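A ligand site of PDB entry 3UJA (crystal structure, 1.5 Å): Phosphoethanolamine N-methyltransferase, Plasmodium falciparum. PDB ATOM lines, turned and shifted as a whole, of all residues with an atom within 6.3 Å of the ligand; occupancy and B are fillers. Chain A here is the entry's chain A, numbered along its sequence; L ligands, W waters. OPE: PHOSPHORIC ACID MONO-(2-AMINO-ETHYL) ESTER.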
ATOM      1  N   GLN A  18      26.349   9.307  17.474  1.00  0.00           N
ATOM      2  CA  GLN A  18      25.690   9.066  18.755  1.00  0.00           C
ATOM      3  C   GLN A  18      24.468   9.959  18.975  1.00  0.00           C
ATOM      4  O   GLN A  18      23.479   9.527  19.565  1.00  0.00           O
ATOM      5  CB  GLN A  18      26.686   9.204  19.905  1.00  0.00           C
ATOM      6  CG  GLN A  18      26.073   8.922  21.274  1.00  0.00           C
ATOM      7  CD  GLN A  18      27.111   8.844  22.366  1.00  0.00           C
ATOM      8  OE1 GLN A  18      28.238   9.302  22.182  1.00  0.00           O
ATOM      9  NE2 GLN A  18      26.732   8.265  23.504  1.00  0.00           N
ATOM     10  N   TYR A  19      24.531  11.204  18.511  1.00  0.00           N
ATOM     11  CA  TYR A  19      23.478  12.162  18.796  1.00  0.00           C
ATOM     12  C   TYR A  19      22.784  12.698  17.550  1.00  0.00           C
ATOM     13  O   TYR A  19      22.519  13.898  17.434  1.00  0.00           O
ATOM     14  CB  TYR A  19      24.012  13.313  19.664  1.00  0.00           C
ATOM     15  CG  TYR A  19      24.573  12.856  21.007  1.00  0.00           C
ATOM     16  CD1 TYR A  19      23.739  12.352  22.005  1.00  0.00           C
ATOM     17  CD2 TYR A  19      25.930  12.917  21.248  1.00  0.00           C
ATOM     18  CE1 TYR A  19      24.262  11.919  23.222  1.00  0.00           C
ATOM     19  CE2 TYR A  19      26.457  12.492  22.461  1.00  0.00           C
ATOM     20  CZ  TYR A  19      25.623  11.999  23.437  1.00  0.00           C
ATOM     21  OH  TYR A  19      26.157  11.590  24.639  1.00  0.00           O
ATOM     22  N   TYR A  27      17.542   7.839  23.357  1.00  0.00           N
ATOM     23  CA  TYR A  27      18.080   8.049  24.685  1.00  0.00           C
ATOM     24  C   TYR A  27      17.003   8.667  25.604  1.00  0.00           C
ATOM     25  O   TYR A  27      16.882   8.277  26.765  1.00  0.00           O
ATOM     26  CB  TYR A  27      19.313   8.960  24.591  1.00  0.00           C
ATOM     27  CG  TYR A  27      20.627   8.233  24.259  1.00  0.00           C
ATOM     28  CD1 TYR A  27      20.953   7.004  24.836  1.00  0.00           C
ATOM     29  CD2 TYR A  27      21.569   8.813  23.411  1.00  0.00           C
ATOM     30  CE1 TYR A  27      22.161   6.367  24.559  1.00  0.00           C
ATOM     31  CE2 TYR A  27      22.770   8.197  23.141  1.00  0.00           C
ATOM     32  CZ  TYR A  27      23.067   6.981  23.716  1.00  0.00           C
ATOM     33  OH  TYR A  27      24.267   6.366  23.446  1.00  0.00           O
ATOM     34  N   PHE A  31      15.998   7.311  29.293  1.00  0.00           N
ATOM     35  CA  PHE A  31      16.420   8.160  30.422  1.00  0.00           C
ATOM     36  C   PHE A  31      15.272   8.941  31.068  1.00  0.00           C
ATOM     37  O   PHE A  31      15.299   9.202  32.277  1.00  0.00           O
ATOM     38  CB  PHE A  31      17.536   9.119  30.008  1.00  0.00           C
ATOM     39  CG  PHE A  31      18.872   8.455  29.783  1.00  0.00           C
ATOM     40  CD1 PHE A  31      19.439   7.658  30.766  1.00  0.00           C
ATOM     41  CD2 PHE A  31      19.551   8.645  28.595  1.00  0.00           C
ATOM     42  CE1 PHE A  31      20.677   7.048  30.548  1.00  0.00           C
ATOM     43  CE2 PHE A  31      20.782   8.050  28.378  1.00  0.00           C
ATOM     44  CZ  PHE A  31      21.349   7.253  29.360  1.00  0.00           C
ATOM     45  N   ILE A  36      19.067  13.089  28.467  1.00  0.00           N
ATOM     46  CA  ILE A  36      19.879  12.122  27.745  1.00  0.00           C
ATOM     47  C   ILE A  36      21.054  11.656  28.597  1.00  0.00           C
ATOM     48  O   ILE A  36      22.026  11.088  28.079  1.00  0.00           O
ATOM     49  CB  ILE A  36      20.361  12.663  26.375  1.00  0.00           C
ATOM     50  CG1 ILE A  36      21.201  13.932  26.544  1.00  0.00           C
ATOM     51  CG2 ILE A  36      19.191  12.922  25.453  1.00  0.00           C
ATOM     52  CD1 ILE A  36      21.723  14.471  25.218  1.00  0.00           C
ATOM     53  N   SER A  37      20.943  11.894  29.903  1.00  0.00           N
ATOM     54  CA  SER A  37      21.972  11.553  30.891  1.00  0.00           C
ATOM     55  C   SER A  37      21.470  10.505  31.884  1.00  0.00           C
ATOM     56  O   SER A  37      20.285  10.458  32.190  1.00  0.00           O
ATOM     57  CB  SER A  37      22.434  12.820  31.646  1.00  0.00           C
ATOM     58  OG  SER A  37      21.345  13.523  32.221  1.00  0.00           O
ATOM     59  N   SER A  38      22.387   9.676  32.401  1.00  0.00           N
ATOM     60  CA  SER A  38      22.081   8.641  33.402  1.00  0.00           C
ATOM     61  C   SER A  38      21.115   9.074  34.492  1.00  0.00           C
ATOM     62  O   SER A  38      21.332  10.080  35.167  1.00  0.00           O
ATOM     63  CB  SER A  38      23.365   8.223  34.134  1.00  0.00           C
ATOM     64  OG  SER A  38      24.432   7.996  33.246  1.00  0.00           O
ATOM     65  N   ARG A 127      26.736  16.899  33.487  1.00  0.00           N
ATOM     66  CA  ARG A 127      26.301  15.520  33.641  1.00  0.00           C
ATOM     67  C   ARG A 127      26.656  14.668  32.434  1.00  0.00           C
ATOM     68  O   ARG A 127      26.048  14.800  31.367  1.00  0.00           O
ATOM     69  CB  ARG A 127      24.786  15.472  33.860  1.00  0.00           C
ATOM     70  CG  ARG A 127      24.293  16.310  35.044  1.00  0.00           C
ATOM     71  CD  ARG A 127      24.788  15.719  36.352  1.00  0.00           C
ATOM     72  NE  ARG A 127      24.389  14.323  36.450  1.00  0.00           N
ATOM     73  CZ  ARG A 127      23.144  13.931  36.742  1.00  0.00           C
ATOM     74  NH1 ARG A 127      22.206  14.830  36.965  1.00  0.00           N
ATOM     75  NH2 ARG A 127      22.858  12.644  36.812  1.00  0.00           N
ATOM     76  N   ASP A 128      27.644  13.783  32.613  1.00  0.00           N
ATOM     77  CA  ASP A 128      27.989  12.757  31.623  1.00  0.00           C
ATOM     78  C   ASP A 128      28.268  13.363  30.260  1.00  0.00           C
ATOM     79  O   ASP A 128      27.769  12.873  29.238  1.00  0.00           O
ATOM     80  CB  ASP A 128      26.874  11.714  31.531  1.00  0.00           C
ATOM     81  CG  ASP A 128      26.614  11.027  32.845  1.00  0.00           C
ATOM     82  OD1 ASP A 128      27.409  11.188  33.808  1.00  0.00           O
ATOM     83  OD2 ASP A 128      25.591  10.309  32.914  1.00  0.00           O
ATOM     84  N   LEU A 131      33.281  13.162  29.220  1.00  0.00           N
ATOM     85  CA  LEU A 131      33.861  11.946  28.638  1.00  0.00           C
ATOM     86  C   LEU A 131      34.208  12.095  27.152  1.00  0.00           C
ATOM     87  O   LEU A 131      35.006  11.322  26.610  1.00  0.00           O
ATOM     88  CB  LEU A 131      32.913  10.757  28.836  1.00  0.00           C
ATOM     89  CG  LEU A 131      31.629  10.652  28.007  1.00  0.00           C
ATOM     90  CD1 LEU A 131      30.944   9.330  28.294  1.00  0.00           C
ATOM     91  CD2 LEU A 131      30.658  11.814  28.266  1.00  0.00           C
ATOM     92  N   HIS A 132      33.577  13.050  26.470  1.00  0.00           N
ATOM     93  CA  HIS A 132      33.834  13.276  25.050  1.00  0.00           C
ATOM     94  C   HIS A 132      35.174  13.983  24.811  1.00  0.00           C
ATOM     95  O   HIS A 132      35.716  13.950  23.695  1.00  0.00           O
ATOM     96  CB  HIS A 132      32.693  14.075  24.406  1.00  0.00           C
ATOM     97  CG  HIS A 132      31.394  13.344  24.353  1.00  0.00           C
ATOM     98  ND1 HIS A 132      31.188  12.245  23.548  1.00  0.00           N
ATOM     99  CD2 HIS A 132      30.228  13.554  25.011  1.00  0.00           C
ATOM    100  CE1 HIS A 132      29.945  11.813  23.707  1.00  0.00           C
ATOM    101  NE2 HIS A 132      29.342  12.584  24.596  1.00  0.00           N
ATOM    102  N   TYR A 160      31.298   9.546  33.103  1.00  0.00           N
ATOM    103  CA  TYR A 160      31.685   8.162  32.921  1.00  0.00           C
ATOM    104  C   TYR A 160      33.172   8.052  33.198  1.00  0.00           C
ATOM    105  O   TYR A 160      33.969   8.844  32.672  1.00  0.00           O
ATOM    106  CB  TYR A 160      31.433   7.718  31.474  1.00  0.00           C
ATOM    107  CG  TYR A 160      29.987   7.417  31.123  1.00  0.00           C
ATOM    108  CD1 TYR A 160      28.933   7.810  31.938  1.00  0.00           C
ATOM    109  CD2 TYR A 160      29.687   6.724  29.946  1.00  0.00           C
ATOM    110  CE1 TYR A 160      27.618   7.514  31.591  1.00  0.00           C
ATOM    111  CE2 TYR A 160      28.385   6.433  29.597  1.00  0.00           C
ATOM    112  CZ  TYR A 160      27.362   6.827  30.416  1.00  0.00           C
ATOM    113  OH  TYR A 160      26.061   6.530  30.059  1.00  0.00           O
ATOM    114  N   TYR A 175      33.832  -0.587  22.804  1.00  0.00           N
ATOM    115  CA  TYR A 175      32.847   0.429  23.184  1.00  0.00           C
ATOM    116  C   TYR A 175      33.487   1.800  23.282  1.00  0.00           C
ATOM    117  O   TYR A 175      33.027   2.760  22.673  1.00  0.00           O
ATOM    118  CB  TYR A 175      32.224   0.029  24.527  1.00  0.00           C
ATOM    119  CG  TYR A 175      31.440   1.090  25.270  1.00  0.00           C
ATOM    120  CD1 TYR A 175      30.154   1.467  24.860  1.00  0.00           C
ATOM    121  CD2 TYR A 175      31.957   1.660  26.423  1.00  0.00           C
ATOM    122  CE1 TYR A 175      29.432   2.420  25.568  1.00  0.00           C
ATOM    123  CE2 TYR A 175      31.240   2.603  27.139  1.00  0.00           C
ATOM    124  CZ  TYR A 175      29.984   2.973  26.701  1.00  0.00           C
ATOM    125  OH  TYR A 175      29.297   3.912  27.451  1.00  0.00           O
ATOM    126  N   ARG A 179      32.765   4.927  20.625  1.00  0.00           N
ATOM    127  CA  ARG A 179      32.181   6.152  21.161  1.00  0.00           C
ATOM    128  C   ARG A 179      33.142   7.332  21.075  1.00  0.00           C
ATOM    129  O   ARG A 179      32.718   8.479  21.189  1.00  0.00           O
ATOM    130  CB  ARG A 179      31.791   5.928  22.622  1.00  0.00           C
ATOM    131  CG  ARG A 179      30.610   4.980  22.853  1.00  0.00           C
ATOM    132  CD  ARG A 179      29.301   5.669  22.520  1.00  0.00           C
ATOM    133  NE  ARG A 179      28.153   4.997  23.141  1.00  0.00           N
ATOM    134  CZ  ARG A 179      27.513   3.951  22.620  1.00  0.00           C
ATOM    135  NH1 ARG A 179      27.872   3.426  21.455  1.00  0.00           N
ATOM    136  NH2 ARG A 179      26.492   3.421  23.292  1.00  0.00           N
ATOM    137  N   TYR A 181      35.232   7.981  23.398  1.00  0.00           N
ATOM    138  CA  TYR A 181      35.345   8.483  24.755  1.00  0.00           C
ATOM    139  C   TYR A 181      36.792   8.463  25.210  1.00  0.00           C
ATOM    140  O   TYR A 181      37.583   7.645  24.751  1.00  0.00           O
ATOM    141  CB  TYR A 181      34.574   7.566  25.708  1.00  0.00           C
ATOM    142  CG  TYR A 181      33.066   7.591  25.619  1.00  0.00           C
ATOM    143  CD1 TYR A 181      32.378   8.651  25.051  1.00  0.00           C
ATOM    144  CD2 TYR A 181      32.323   6.534  26.139  1.00  0.00           C
ATOM    145  CE1 TYR A 181      30.988   8.652  25.010  1.00  0.00           C
ATOM    146  CE2 TYR A 181      30.950   6.537  26.113  1.00  0.00           C
ATOM    147  CZ  TYR A 181      30.294   7.598  25.549  1.00  0.00           C
ATOM    148  OH  TYR A 181      28.919   7.575  25.542  1.00  0.00           O
ATOM    149  N   TRP A 210      24.851   3.877  40.094  1.00  0.00           N
ATOM    150  CA  TRP A 210      24.683   3.907  38.655  1.00  0.00           C
ATOM    151  C   TRP A 210      24.075   2.587  38.157  1.00  0.00           C
ATOM    152  O   TRP A 210      23.192   2.567  37.301  1.00  0.00           O
ATOM    153  CB  TRP A 210      26.023   4.188  37.981  1.00  0.00           C
ATOM    154  CG  TRP A 210      25.948   4.512  36.524  1.00  0.00           C
ATOM    155  CD1 TRP A 210      25.202   5.503  35.948  1.00  0.00           C
ATOM    156  CD2 TRP A 210      26.653   3.859  35.459  1.00  0.00           C
ATOM    157  NE1 TRP A 210      25.405   5.502  34.578  1.00  0.00           N
ATOM    158  CE2 TRP A 210      26.286   4.501  34.259  1.00  0.00           C
ATOM    159  CE3 TRP A 210      27.564   2.792  35.410  1.00  0.00           C
ATOM    160  CZ2 TRP A 210      26.793   4.111  33.016  1.00  0.00           C
ATOM    161  CZ3 TRP A 210      28.071   2.402  34.167  1.00  0.00           C
ATOM    162  CH2 TRP A 210      27.691   3.064  32.987  1.00  0.00           C
ATOM    163  N   TRP A 244      22.615  -1.453  27.414  1.00  0.00           N
ATOM    164  CA  TRP A 244      22.344  -1.340  28.842  1.00  0.00           C
ATOM    165  C   TRP A 244      22.808  -2.608  29.557  1.00  0.00           C
ATOM    166  O   TRP A 244      23.349  -2.529  30.656  1.00  0.00           O
ATOM    167  CB  TRP A 244      20.859  -1.062  29.120  1.00  0.00           C
ATOM    168  CG  TRP A 244      20.585   0.369  29.511  1.00  0.00           C
ATOM    169  CD1 TRP A 244      20.092   0.802  30.712  1.00  0.00           C
ATOM    170  CD2 TRP A 244      20.803   1.542  28.707  1.00  0.00           C
ATOM    171  NE1 TRP A 244      19.993   2.168  30.711  1.00  0.00           N
ATOM    172  CE2 TRP A 244      20.426   2.643  29.496  1.00  0.00           C
ATOM    173  CE3 TRP A 244      21.293   1.757  27.420  1.00  0.00           C
ATOM    174  CZ2 TRP A 244      20.507   3.958  29.032  1.00  0.00           C
ATOM    175  CZ3 TRP A 244      21.376   3.066  26.948  1.00  0.00           C
ATOM    176  CH2 TRP A 244      20.978   4.152  27.758  1.00  0.00           C
ATOM    177  N   ARG A 246      25.355  -4.458  28.865  1.00  0.00           N
ATOM    178  CA  ARG A 246      26.797  -4.396  29.054  1.00  0.00           C
ATOM    179  C   ARG A 246      27.173  -3.398  30.140  1.00  0.00           C
ATOM    180  O   ARG A 246      28.089  -3.655  30.919  1.00  0.00           O
ATOM    181  CB  ARG A 246      27.553  -4.039  27.765  1.00  0.00           C
ATOM    182  CG  ARG A 246      29.067  -4.178  27.941  1.00  0.00           C
ATOM    183  CD  ARG A 246      29.873  -3.309  26.979  1.00  0.00           C
ATOM    184  NE  ARG A 246      29.419  -1.940  26.996  1.00  0.00           N
ATOM    185  CZ  ARG A 246      29.731  -1.036  27.916  1.00  0.00           C
ATOM    186  NH1 ARG A 246      30.541  -1.337  28.939  1.00  0.00           N
ATOM    187  NH2 ARG A 246      29.219   0.174  27.829  1.00  0.00           N
ATOM    188  N   LYS A 247      26.501  -2.256  30.182  1.00  0.00           N
ATOM    189  CA  LYS A 247      26.806  -1.283  31.237  1.00  0.00           C
ATOM    190  C   LYS A 247      26.459  -1.829  32.620  1.00  0.00           C
ATOM    191  O   LYS A 247      27.141  -1.540  33.594  1.00  0.00           O
ATOM    192  CB  LYS A 247      26.078   0.039  31.007  1.00  0.00           C
ATOM    193  CG  LYS A 247      26.654   0.870  29.861  1.00  0.00           C
ATOM    194  CD  LYS A 247      25.952   2.226  29.737  1.00  0.00           C
ATOM    195  CE  LYS A 247      24.535   2.087  29.204  1.00  0.00           C
ATOM    196  NZ  LYS A 247      23.937   3.440  28.997  1.00  0.00           N
ATOM    197  N   GLN A 256      33.530  -0.394  34.087  1.00  0.00           N
ATOM    198  CA  GLN A 256      33.025   0.931  33.751  1.00  0.00           C
ATOM    199  C   GLN A 256      32.456   1.522  35.035  1.00  0.00           C
ATOM    200  O   GLN A 256      31.700   0.865  35.730  1.00  0.00           O
ATOM    201  CB  GLN A 256      31.964   0.886  32.634  1.00  0.00           C
ATOM    202  CG  GLN A 256      31.537   2.277  32.185  1.00  0.00           C
ATOM    203  CD  GLN A 256      30.667   2.282  30.933  1.00  0.00           C
ATOM    204  OE1 GLN A 256      30.382   1.238  30.364  1.00  0.00           O
ATOM    205  NE2 GLN A 256      30.242   3.475  30.520  1.00  0.00           N
HETATM  206  CA  OPE L   1      24.710   7.638  26.861  1.00  0.00           C
HETATM  207  CB  OPE L   1      24.501   9.119  26.757  1.00  0.00           C
HETATM  208  O1  OPE L   1      25.159   4.890  25.410  1.00  0.00           O
HETATM  209  O2  OPE L   1      25.800   5.162  27.806  1.00  0.00           O
HETATM  210  O3  OPE L   1      27.601   5.433  26.049  1.00  0.00           O
HETATM  211  O4  OPE L   1      25.855   7.086  26.358  1.00  0.00           O
HETATM  212  N   OPE L   1      25.321   9.932  27.622  1.00  0.00           N
HETATM  213  P   OPE L   1      26.122   5.546  26.377  1.00  0.00           P
HETATM  214  O   HOH W   1      24.734   9.131  30.260  1.00  0.00           O
HETATM  215  O   HOH W   2      24.615   2.279  25.823  1.00  0.00           O
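NE2 of Gln 18 sits at hydrogen-bond distance from OH of Tyr 27.
The side-chain hydroxyl (OH) of Tyr 181 is in hydrogen-bond range of the side-chain amide nitrogen (NE2) of Gln 18 (3.1 Å).
The side-chain hydroxyl (OH) of Tyr 19 lies within hydrogen-bond range of a ring nitrogen (NE2) of His 132, 3.3 Å away.
The side-chain hydroxyl of Tyr 175 is in hydrogen-bond range of the side-chain amide nitrogen of Gln 256.
Water W2 lies within hydrogen-bond range of O1 of the ligand (2.7 Å), NH2 of Arg 179 (3.4 Å) and NZ of Lys 247 (3.4 Å).
Water W1 lies within hydrogen-bond range of a nitrogen (N) of the ligand (2.8 Å), the side-chain hydroxyl of Tyr 160 (2.9 Å), the side-chain carboxylate of Asp 128 (3.0 Å) and the side-chain hydroxyl of Ser 38 (3.2 Å).
An oxygen (O2) of the ligand lies within salt-bridge range of the side-chain amino group of Lys 247 (2.8 Å).
OH of Tyr 27 lies within hydrogen-bond range of O1 of the ligand, at 2.6 Å.
The side-chain hydroxyl of Tyr 181 lies within hydrogen-bond range of an oxygen (O3) of the ligand (2.6 Å).
The side-chain hydroxyl (OH) of Tyr 175 lies within hydrogen-bond range of an oxygen (O3) of the ligand (2.7 Å).
O4 of the ligand is in hydrogen-bond range of NE2 of Gln 18 (3.2 Å).
NH2 of Arg 179 is in salt-bridge range of O1 of the ligand.
OH of Tyr 160 sits at hydrogen-bond distance from O2 of the ligand (2.6 Å).
Residues that only touch the ligand: Tyr 19 and Ile 36.
Hydrophobic or aromatic side chains that line the ligand: Tyr 27, Tyr 160, Tyr 175 and Tyr 181.
Within 4 Å of the ligand: Gln 18, Tyr 19, Tyr 27, Ile 36, Tyr 160, Tyr 175, Arg 179, Tyr 181 and Lys 247.
Along chain A the residues within 4 Å of the ligand span positions 18 to 247.
The nearest printed residue that does not touch the ligand is Asp 128 (4.2 Å).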
